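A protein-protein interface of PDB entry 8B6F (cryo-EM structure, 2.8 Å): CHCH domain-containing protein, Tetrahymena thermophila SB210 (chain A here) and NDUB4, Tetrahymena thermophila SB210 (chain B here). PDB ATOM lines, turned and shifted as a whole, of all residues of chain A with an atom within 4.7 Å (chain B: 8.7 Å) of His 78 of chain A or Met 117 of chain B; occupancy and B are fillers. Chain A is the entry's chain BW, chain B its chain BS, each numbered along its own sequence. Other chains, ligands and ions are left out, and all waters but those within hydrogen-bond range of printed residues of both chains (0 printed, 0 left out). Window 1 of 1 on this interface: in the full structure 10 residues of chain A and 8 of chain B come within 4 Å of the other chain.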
ATOM      1  N   TRP A   7       8.946  17.835  10.944  1.00  0.00           N
ATOM      2  CA  TRP A   7       8.515  16.513  10.504  1.00  0.00           C
ATOM      3  C   TRP A   7       8.955  15.407  11.454  1.00  0.00           C
ATOM      4  O   TRP A   7       8.339  14.335  11.459  1.00  0.00           O
ATOM      5  CB  TRP A   7       9.036  16.227   9.092  1.00  0.00           C
ATOM      6  CG  TRP A   7      10.513  16.413   8.917  1.00  0.00           C
ATOM      7  CD1 TRP A   7      11.151  17.549   8.519  1.00  0.00           C
ATOM      8  CD2 TRP A   7      11.536  15.429   9.120  1.00  0.00           C
ATOM      9  NE1 TRP A   7      12.506  17.336   8.465  1.00  0.00           N
ATOM     10  CE2 TRP A   7      12.767  16.043   8.830  1.00  0.00           C
ATOM     11  CE3 TRP A   7      11.526  14.091   9.523  1.00  0.00           C
ATOM     12  CZ2 TRP A   7      13.980  15.365   8.931  1.00  0.00           C
ATOM     13  CZ3 TRP A   7      12.731  13.418   9.621  1.00  0.00           C
ATOM     14  CH2 TRP A   7      13.942  14.058   9.328  1.00  0.00           C
ATOM     15  N   THR A  74       4.777  11.261   7.332  1.00  0.00           N
ATOM     16  CA  THR A  74       5.521  12.462   6.970  1.00  0.00           C
ATOM     17  C   THR A  74       6.988  12.317   7.349  1.00  0.00           C
ATOM     18  O   THR A  74       7.883  12.643   6.562  1.00  0.00           O
ATOM     19  CB  THR A  74       4.908  13.686   7.650  1.00  0.00           C
ATOM     20  OG1 THR A  74       3.522  13.787   7.305  1.00  0.00           O
ATOM     21  CG2 THR A  74       5.630  14.954   7.217  1.00  0.00           C
ATOM     22  N   CYS A  75       7.254  11.834   8.564  1.00  0.00           N
ATOM     23  CA  CYS A  75       8.632  11.661   9.004  1.00  0.00           C
ATOM     24  C   CYS A  75       9.354  10.643   8.135  1.00  0.00           C
ATOM     25  O   CYS A  75      10.523  10.833   7.779  1.00  0.00           O
ATOM     26  CB  CYS A  75       8.671  11.239  10.473  1.00  0.00           C
ATOM     27  SG  CYS A  75      10.325  11.300  11.192  1.00  0.00           S
ATOM     28  N   LEU A  76       8.671   9.554   7.781  1.00  0.00           N
ATOM     29  CA  LEU A  76       9.283   8.535   6.936  1.00  0.00           C
ATOM     30  C   LEU A  76       9.622   9.093   5.560  1.00  0.00           C
ATOM     31  O   LEU A  76      10.704   8.826   5.025  1.00  0.00           O
ATOM     32  CB  LEU A  76       8.353   7.327   6.818  1.00  0.00           C
ATOM     33  CG  LEU A  76       8.851   6.159   5.965  1.00  0.00           C
ATOM     34  CD1 LEU A  76      10.075   5.511   6.598  1.00  0.00           C
ATOM     35  CD2 LEU A  76       7.745   5.139   5.766  1.00  0.00           C
ATOM     36  N   ASN A  77       8.712   9.868   4.967  1.00  0.00           N
ATOM     37  CA  ASN A  77       8.998  10.470   3.670  1.00  0.00           C
ATOM     38  C   ASN A  77      10.241  11.350   3.738  1.00  0.00           C
ATOM     39  O   ASN A  77      11.143  11.235   2.902  1.00  0.00           O
ATOM     40  CB  ASN A  77       7.795  11.282   3.191  1.00  0.00           C
ATOM     41  CG  ASN A  77       6.613  10.411   2.826  1.00  0.00           C
ATOM     42  OD1 ASN A  77       6.770   9.232   2.513  1.00  0.00           O
ATOM     43  ND2 ASN A  77       5.418  10.988   2.864  1.00  0.00           N
ATOM     44  N   HIS A  78      10.304  12.240   4.730  1.00  0.00           N
ATOM     45  CA  HIS A  78      11.460  13.121   4.848  1.00  0.00           C
ATOM     46  C   HIS A  78      12.733  12.325   5.094  1.00  0.00           C
ATOM     47  O   HIS A  78      13.780  12.614   4.505  1.00  0.00           O
ATOM     48  CB  HIS A  78      11.236  14.134   5.968  1.00  0.00           C
ATOM     49  CG  HIS A  78      10.345  15.272   5.578  1.00  0.00           C
ATOM     50  ND1 HIS A  78       8.979  15.138   5.454  1.00  0.00           N
ATOM     51  CD2 HIS A  78      10.626  16.560   5.276  1.00  0.00           C
ATOM     52  CE1 HIS A  78       8.457  16.297   5.096  1.00  0.00           C
ATOM     53  NE2 HIS A  78       9.435  17.177   4.980  1.00  0.00           N
ATOM     54  N   TRP A  79      12.661  11.317   5.965  1.00  0.00           N
ATOM     55  CA  TRP A  79      13.839  10.516   6.278  1.00  0.00           C
ATOM     56  C   TRP A  79      14.392   9.842   5.029  1.00  0.00           C
ATOM     57  O   TRP A  79      15.591   9.930   4.741  1.00  0.00           O
ATOM     58  CB  TRP A  79      13.475   9.480   7.342  1.00  0.00           C
ATOM     59  CG  TRP A  79      14.537   8.467   7.626  1.00  0.00           C
ATOM     60  CD1 TRP A  79      15.884   8.616   7.475  1.00  0.00           C
ATOM     61  CD2 TRP A  79      14.334   7.136   8.116  1.00  0.00           C
ATOM     62  NE1 TRP A  79      16.531   7.461   7.840  1.00  0.00           N
ATOM     63  CE2 TRP A  79      15.600   6.537   8.238  1.00  0.00           C
ATOM     64  CE3 TRP A  79      13.199   6.396   8.464  1.00  0.00           C
ATOM     65  CZ2 TRP A  79      15.767   5.231   8.692  1.00  0.00           C
ATOM     66  CZ3 TRP A  79      13.366   5.099   8.915  1.00  0.00           C
ATOM     67  CH2 TRP A  79      14.641   4.529   9.026  1.00  0.00           C
ATOM     68  N   GLN A  80      13.532   9.156   4.276  1.00  0.00           N
ATOM     69  CA  GLN A  80      14.001   8.435   3.096  1.00  0.00           C
ATOM     70  C   GLN A  80      14.464   9.392   2.005  1.00  0.00           C
ATOM     71  O   GLN A  80      15.453   9.122   1.315  1.00  0.00           O
ATOM     72  CB  GLN A  80      12.902   7.513   2.574  1.00  0.00           C
ATOM     73  CG  GLN A  80      12.417   6.501   3.597  1.00  0.00           C
ATOM     74  CD  GLN A  80      13.522   5.591   4.093  1.00  0.00           C
ATOM     75  OE1 GLN A  80      14.606   5.537   3.518  1.00  0.00           O
ATOM     76  NE2 GLN A  80      13.249   4.867   5.172  1.00  0.00           N
ATOM     77  N   THR A  81      13.761  10.514   1.827  1.00  0.00           N
ATOM     78  CA  THR A  81      14.176  11.485   0.820  1.00  0.00           C
ATOM     79  C   THR A  81      15.561  12.039   1.127  1.00  0.00           C
ATOM     80  O   THR A  81      16.390  12.192   0.222  1.00  0.00           O
ATOM     81  CB  THR A  81      13.156  12.619   0.732  1.00  0.00           C
ATOM     82  OG1 THR A  81      11.879  12.091   0.357  1.00  0.00           O
ATOM     83  CG2 THR A  81      13.590  13.654  -0.296  1.00  0.00           C
ATOM     84  N   TYR A  82      15.831  12.354   2.394  1.00  0.00           N
ATOM     85  CA  TYR A  82      17.146  12.868   2.755  1.00  0.00           C
ATOM     86  C   TYR A  82      18.205  11.776   2.714  1.00  0.00           C
ATOM     87  O   TYR A  82      19.378  12.066   2.460  1.00  0.00           O
ATOM     88  CB  TYR A  82      17.102  13.509   4.143  1.00  0.00           C
ATOM     89  CG  TYR A  82      16.168  14.695   4.244  1.00  0.00           C
ATOM     90  CD1 TYR A  82      15.910  15.500   3.142  1.00  0.00           C
ATOM     91  CD2 TYR A  82      15.539  15.006   5.441  1.00  0.00           C
ATOM     92  CE1 TYR A  82      15.057  16.577   3.230  1.00  0.00           C
ATOM     93  CE2 TYR A  82      14.683  16.084   5.539  1.00  0.00           C
ATOM     94  CZ  TYR A  82      14.446  16.866   4.428  1.00  0.00           C
ATOM     95  OH  TYR A  82      13.595  17.941   4.517  1.00  0.00           O
ATOM     96  N   HIS A  87      15.281  14.253  -3.582  1.00  0.00           N
ATOM     97  CA  HIS A  87      14.705  15.556  -3.898  1.00  0.00           C
ATOM     98  C   HIS A  87      15.623  16.363  -4.806  1.00  0.00           C
ATOM     99  O   HIS A  87      15.147  17.214  -5.566  1.00  0.00           O
ATOM    100  CB  HIS A  87      14.397  16.331  -2.614  1.00  0.00           C
ATOM    101  CG  HIS A  87      15.602  16.641  -1.781  1.00  0.00           C
ATOM    102  ND1 HIS A  87      16.229  15.698  -0.996  1.00  0.00           N
ATOM    103  CD2 HIS A  87      16.281  17.796  -1.593  1.00  0.00           C
ATOM    104  CE1 HIS A  87      17.250  16.256  -0.371  1.00  0.00           C
ATOM    105  NE2 HIS A  87      17.302  17.530  -0.714  1.00  0.00           N
ATOM    106  N   LYS B 110       1.552  23.211  -3.042  1.00  0.00           N
ATOM    107  CA  LYS B 110       2.586  22.453  -3.737  1.00  0.00           C
ATOM    108  C   LYS B 110       3.952  23.090  -3.527  1.00  0.00           C
ATOM    109  O   LYS B 110       4.931  22.402  -3.219  1.00  0.00           O
ATOM    110  CB  LYS B 110       2.255  22.360  -5.225  1.00  0.00           C
ATOM    111  CG  LYS B 110       1.053  21.481  -5.528  1.00  0.00           C
ATOM    112  CD  LYS B 110       0.713  21.469  -7.012  1.00  0.00           C
ATOM    113  CE  LYS B 110       1.862  20.946  -7.859  1.00  0.00           C
ATOM    114  NZ  LYS B 110       2.374  19.632  -7.383  1.00  0.00           N
ATOM    115  N   LEU B 111       4.041  24.411  -3.694  1.00  0.00           N
ATOM    116  CA  LEU B 111       5.318  25.084  -3.493  1.00  0.00           C
ATOM    117  C   LEU B 111       5.785  24.948  -2.051  1.00  0.00           C
ATOM    118  O   LEU B 111       6.976  24.745  -1.792  1.00  0.00           O
ATOM    119  CB  LEU B 111       5.225  26.558  -3.882  1.00  0.00           C
ATOM    120  CG  LEU B 111       6.552  27.270  -3.617  1.00  0.00           C
ATOM    121  CD1 LEU B 111       7.010  28.049  -4.812  1.00  0.00           C
ATOM    122  CD2 LEU B 111       6.411  28.195  -2.416  1.00  0.00           C
ATOM    123  N   ASP B 112       4.856  25.040  -1.098  1.00  0.00           N
ATOM    124  CA  ASP B 112       5.225  24.913   0.308  1.00  0.00           C
ATOM    125  C   ASP B 112       5.778  23.528   0.600  1.00  0.00           C
ATOM    126  O   ASP B 112       6.761  23.387   1.337  1.00  0.00           O
ATOM    127  CB  ASP B 112       4.019  25.206   1.198  1.00  0.00           C
ATOM    128  CG  ASP B 112       3.577  26.654   1.121  1.00  0.00           C
ATOM    129  OD1 ASP B 112       4.229  27.436   0.399  1.00  0.00           O
ATOM    130  OD2 ASP B 112       2.579  27.011   1.781  1.00  0.00           O
ATOM    131  N   GLY B 113       5.160  22.490   0.040  1.00  0.00           N
ATOM    132  CA  GLY B 113       5.701  21.154   0.215  1.00  0.00           C
ATOM    133  C   GLY B 113       7.104  21.030  -0.342  1.00  0.00           C
ATOM    134  O   GLY B 113       7.992  20.459   0.295  1.00  0.00           O
ATOM    135  N   PHE B 114       7.324  21.562  -1.546  1.00  0.00           N
ATOM    136  CA  PHE B 114       8.647  21.492  -2.159  1.00  0.00           C
ATOM    137  C   PHE B 114       9.690  22.202  -1.302  1.00  0.00           C
ATOM    138  O   PHE B 114      10.756  21.645  -1.013  1.00  0.00           O
ATOM    139  CB  PHE B 114       8.592  22.099  -3.562  1.00  0.00           C
ATOM    140  CG  PHE B 114       9.901  22.065  -4.295  1.00  0.00           C
ATOM    141  CD1 PHE B 114      10.374  20.881  -4.834  1.00  0.00           C
ATOM    142  CD2 PHE B 114      10.650  23.216  -4.457  1.00  0.00           C
ATOM    143  CE1 PHE B 114      11.574  20.844  -5.515  1.00  0.00           C
ATOM    144  CE2 PHE B 114      11.853  23.186  -5.138  1.00  0.00           C
ATOM    145  CZ  PHE B 114      12.315  21.997  -5.668  1.00  0.00           C
ATOM    146  N   VAL B 115       9.402  23.435  -0.882  1.00  0.00           N
ATOM    147  CA  VAL B 115      10.386  24.207  -0.127  1.00  0.00           C
ATOM    148  C   VAL B 115      10.621  23.584   1.243  1.00  0.00           C
ATOM    149  O   VAL B 115      11.747  23.579   1.753  1.00  0.00           O
ATOM    150  CB  VAL B 115       9.955  25.682  -0.011  1.00  0.00           C
ATOM    151  CG1 VAL B 115       9.819  26.307  -1.388  1.00  0.00           C
ATOM    152  CG2 VAL B 115       8.662  25.810   0.771  1.00  0.00           C
ATOM    153  N   SER B 116       9.567  23.047   1.861  1.00  0.00           N
ATOM    154  CA  SER B 116       9.733  22.395   3.155  1.00  0.00           C
ATOM    155  C   SER B 116      10.610  21.157   3.037  1.00  0.00           C
ATOM    156  O   SER B 116      11.474  20.917   3.887  1.00  0.00           O
ATOM    157  CB  SER B 116       8.368  22.032   3.739  1.00  0.00           C
ATOM    158  OG  SER B 116       7.678  21.124   2.897  1.00  0.00           O
ATOM    159  N   MET B 117      10.399  20.355   1.993  1.00  0.00           N
ATOM    160  CA  MET B 117      11.257  19.195   1.788  1.00  0.00           C
ATOM    161  C   MET B 117      12.708  19.616   1.604  1.00  0.00           C
ATOM    162  O   MET B 117      13.620  18.983   2.149  1.00  0.00           O
ATOM    163  CB  MET B 117      10.771  18.399   0.576  1.00  0.00           C
ATOM    164  CG  MET B 117      11.646  17.211   0.214  1.00  0.00           C
ATOM    165  SD  MET B 117      11.842  16.038   1.567  1.00  0.00           S
ATOM    166  CE  MET B 117      10.175  15.406   1.712  1.00  0.00           C
ATOM    167  N   PHE B 118      12.945  20.683   0.839  1.00  0.00           N
ATOM    168  CA  PHE B 118      14.313  21.133   0.605  1.00  0.00           C
ATOM    169  C   PHE B 118      14.940  21.702   1.874  1.00  0.00           C
ATOM    170  O   PHE B 118      16.128  21.486   2.135  1.00  0.00           O
ATOM    171  CB  PHE B 118      14.341  22.164  -0.522  1.00  0.00           C
ATOM    172  CG  PHE B 118      14.792  21.601  -1.838  1.00  0.00           C
ATOM    173  CD1 PHE B 118      13.991  20.710  -2.533  1.00  0.00           C
ATOM    174  CD2 PHE B 118      16.016  21.954  -2.375  1.00  0.00           C
ATOM    175  CE1 PHE B 118      14.402  20.187  -3.741  1.00  0.00           C
ATOM    176  CE2 PHE B 118      16.433  21.433  -3.585  1.00  0.00           C
ATOM    177  CZ  PHE B 118      15.625  20.549  -4.268  1.00  0.00           C
ATOM    178  N   LYS B 119      14.161  22.439   2.670  1.00  0.00           N
ATOM    179  CA  LYS B 119      14.724  23.115   3.836  1.00  0.00           C
ATOM    180  C   LYS B 119      14.968  22.157   4.995  1.00  0.00           C
ATOM    181  O   LYS B 119      15.961  22.296   5.716  1.00  0.00           O
ATOM    182  CB  LYS B 119      13.796  24.242   4.290  1.00  0.00           C
ATOM    183  CG  LYS B 119      13.744  25.433   3.353  1.00  0.00           C
ATOM    184  CD  LYS B 119      12.752  26.471   3.850  1.00  0.00           C
ATOM    185  CE  LYS B 119      12.680  27.659   2.907  1.00  0.00           C
ATOM    186  NZ  LYS B 119      11.643  28.639   3.330  1.00  0.00           N
ATOM    187  N   GLY B 120      14.082  21.184   5.190  1.00  0.00           N
ATOM    188  CA  GLY B 120      14.112  20.373   6.393  1.00  0.00           C
ATOM    189  C   GLY B 120      15.228  19.350   6.454  1.00  0.00           C
ATOM    190  O   GLY B 120      15.164  18.417   7.259  1.00  0.00           O
ATOM    191  N   SER B 121      16.259  19.508   5.622  1.00  0.00           N
ATOM    192  CA  SER B 121      17.342  18.532   5.602  1.00  0.00           C
ATOM    193  C   SER B 121      18.083  18.482   6.931  1.00  0.00           C
ATOM    194  O   SER B 121      18.636  17.437   7.292  1.00  0.00           O
ATOM    195  CB  SER B 121      18.313  18.850   4.467  1.00  0.00           C
ATOM    196  OG  SER B 121      18.903  20.125   4.641  1.00  0.00           O
ATOM    197  N   ASP B 122      18.111  19.591   7.668  1.00  0.00           N
ATOM    198  CA  ASP B 122      18.871  19.698   8.905  1.00  0.00           C
ATOM    199  C   ASP B 122      18.001  19.557  10.149  1.00  0.00           C
ATOM    200  O   ASP B 122      18.467  19.853  11.253  1.00  0.00           O
ATOM    201  CB  ASP B 122      19.614  21.035   8.940  1.00  0.00           C
ATOM    202  CG  ASP B 122      20.705  21.072   9.992  1.00  0.00           C
ATOM    203  OD1 ASP B 122      20.963  20.026  10.622  1.00  0.00           O
ATOM    204  OD2 ASP B 122      21.305  22.150  10.193  1.00  0.00           O
ATOM    205  N   VAL B 123      16.751  19.114  10.003  1.00  0.00           N
ATOM    206  CA  VAL B 123      15.877  18.982  11.167  1.00  0.00           C
ATOM    207  C   VAL B 123      16.440  17.956  12.142  1.00  0.00           C
ATOM    208  O   VAL B 123      16.435  18.170  13.361  1.00  0.00           O
ATOM    209  CB  VAL B 123      14.447  18.621  10.723  1.00  0.00           C
ATOM    210  CG1 VAL B 123      13.588  18.218  11.918  1.00  0.00           C
ATOM    211  CG2 VAL B 123      13.815  19.789   9.992  1.00  0.00           C
ATOM    212  N   ALA B 124      16.922  16.828  11.630  1.00  0.00           N
ATOM    213  CA  ALA B 124      17.471  15.772  12.474  1.00  0.00           C
ATOM    214  C   ALA B 124      18.918  16.107  12.812  1.00  0.00           C
ATOM    215  O   ALA B 124      19.786  16.101  11.933  1.00  0.00           O
ATOM    216  CB  ALA B 124      17.372  14.423  11.771  1.00  0.00           C
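O of Gly 120 of chain B sits close to OH of Tyr 82 of chain A (3.2 Å). N of Ser 121 of chain B sits at hydrogen-bond distance from OH of Tyr 82 of chain A, at 3.3 Å. O of Met 117 of chain B is in hydrogen-bond range of OH of Tyr 82 of chain A (2.6 Å). The backbone carbonyl oxygen (O) of Gly 120 of chain B is in hydrogen-bond range of the indole nitrogen (NE1) of Trp 7 of chain A.
The backbone carbonyl oxygen (O) of Gly 113 of chain B lies within hydrogen-bond range of the side-chain hydroxyl (OG) of Ser 116 of chain B, 2.7 Å away. The backbone carbonyl oxygen (O) of Asp 112 of chain B is in hydrogen-bond range of the side-chain hydroxyl (OG) of Ser 116 of chain B, 2.9 Å away. The backbone carbonyl oxygen of Thr 74 of chain A lies within hydrogen-bond range of a ring nitrogen (ND1) of His 78 of chain A, 2.9 Å away. The backbone carbonyl oxygen (O) of Asn 77 of chain A sits at hydrogen-bond distance from the side-chain hydroxyl (OG1) of Thr 81 of chain A.
Among the printed residues, pairs that only touch across the chains: Trp 7 of chain A with Val 123 of chain B (3.2 Å), Thr 81 of chain A with Met 117 of chain B (3.5 Å), His 87 of chain A with Phe 118 of chain B (3.6 Å), Tyr 82 of chain A with Ser 116 of chain B (3.7 Å) and His 78 of chain A with Met 117 of chain B (3.8 Å).
Of the printed residues of chain B, Trp 7 of chain A touches Gly 120 (3.1 Å) and Val 123 (3.2 Å). His 78 of chain A touches just one residue of chain B: Met 117. Of chain A, only His 78, Thr 81 and Tyr 82 come within 4 Å of Met 117 of chain B. Of the printed residues of chain A, Ser 121 of chain B touches Tyr 82 (3.3 Å). The nearest residue of chain B that does not touch His 78 of chain A is Ser 116 of chain B (4.4 Å).
Hydrophobic or aromatic side chains of chain A within 4 Å of the printed part of chain B: Trp 7, His 78, Tyr 82 and His 87. Of the 15 printed residues of chain B, 6 touch a printed residue of chain A. Printed residues of chain B that touch a printed residue of chain A: Ser 116, Met 117, Phe 118, Gly 120, Ser 121 and Val 123. Hydrophobic or aromatic side chains of chain B that line the printed part of chain A: Met 117, Phe 118 and Val 123.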
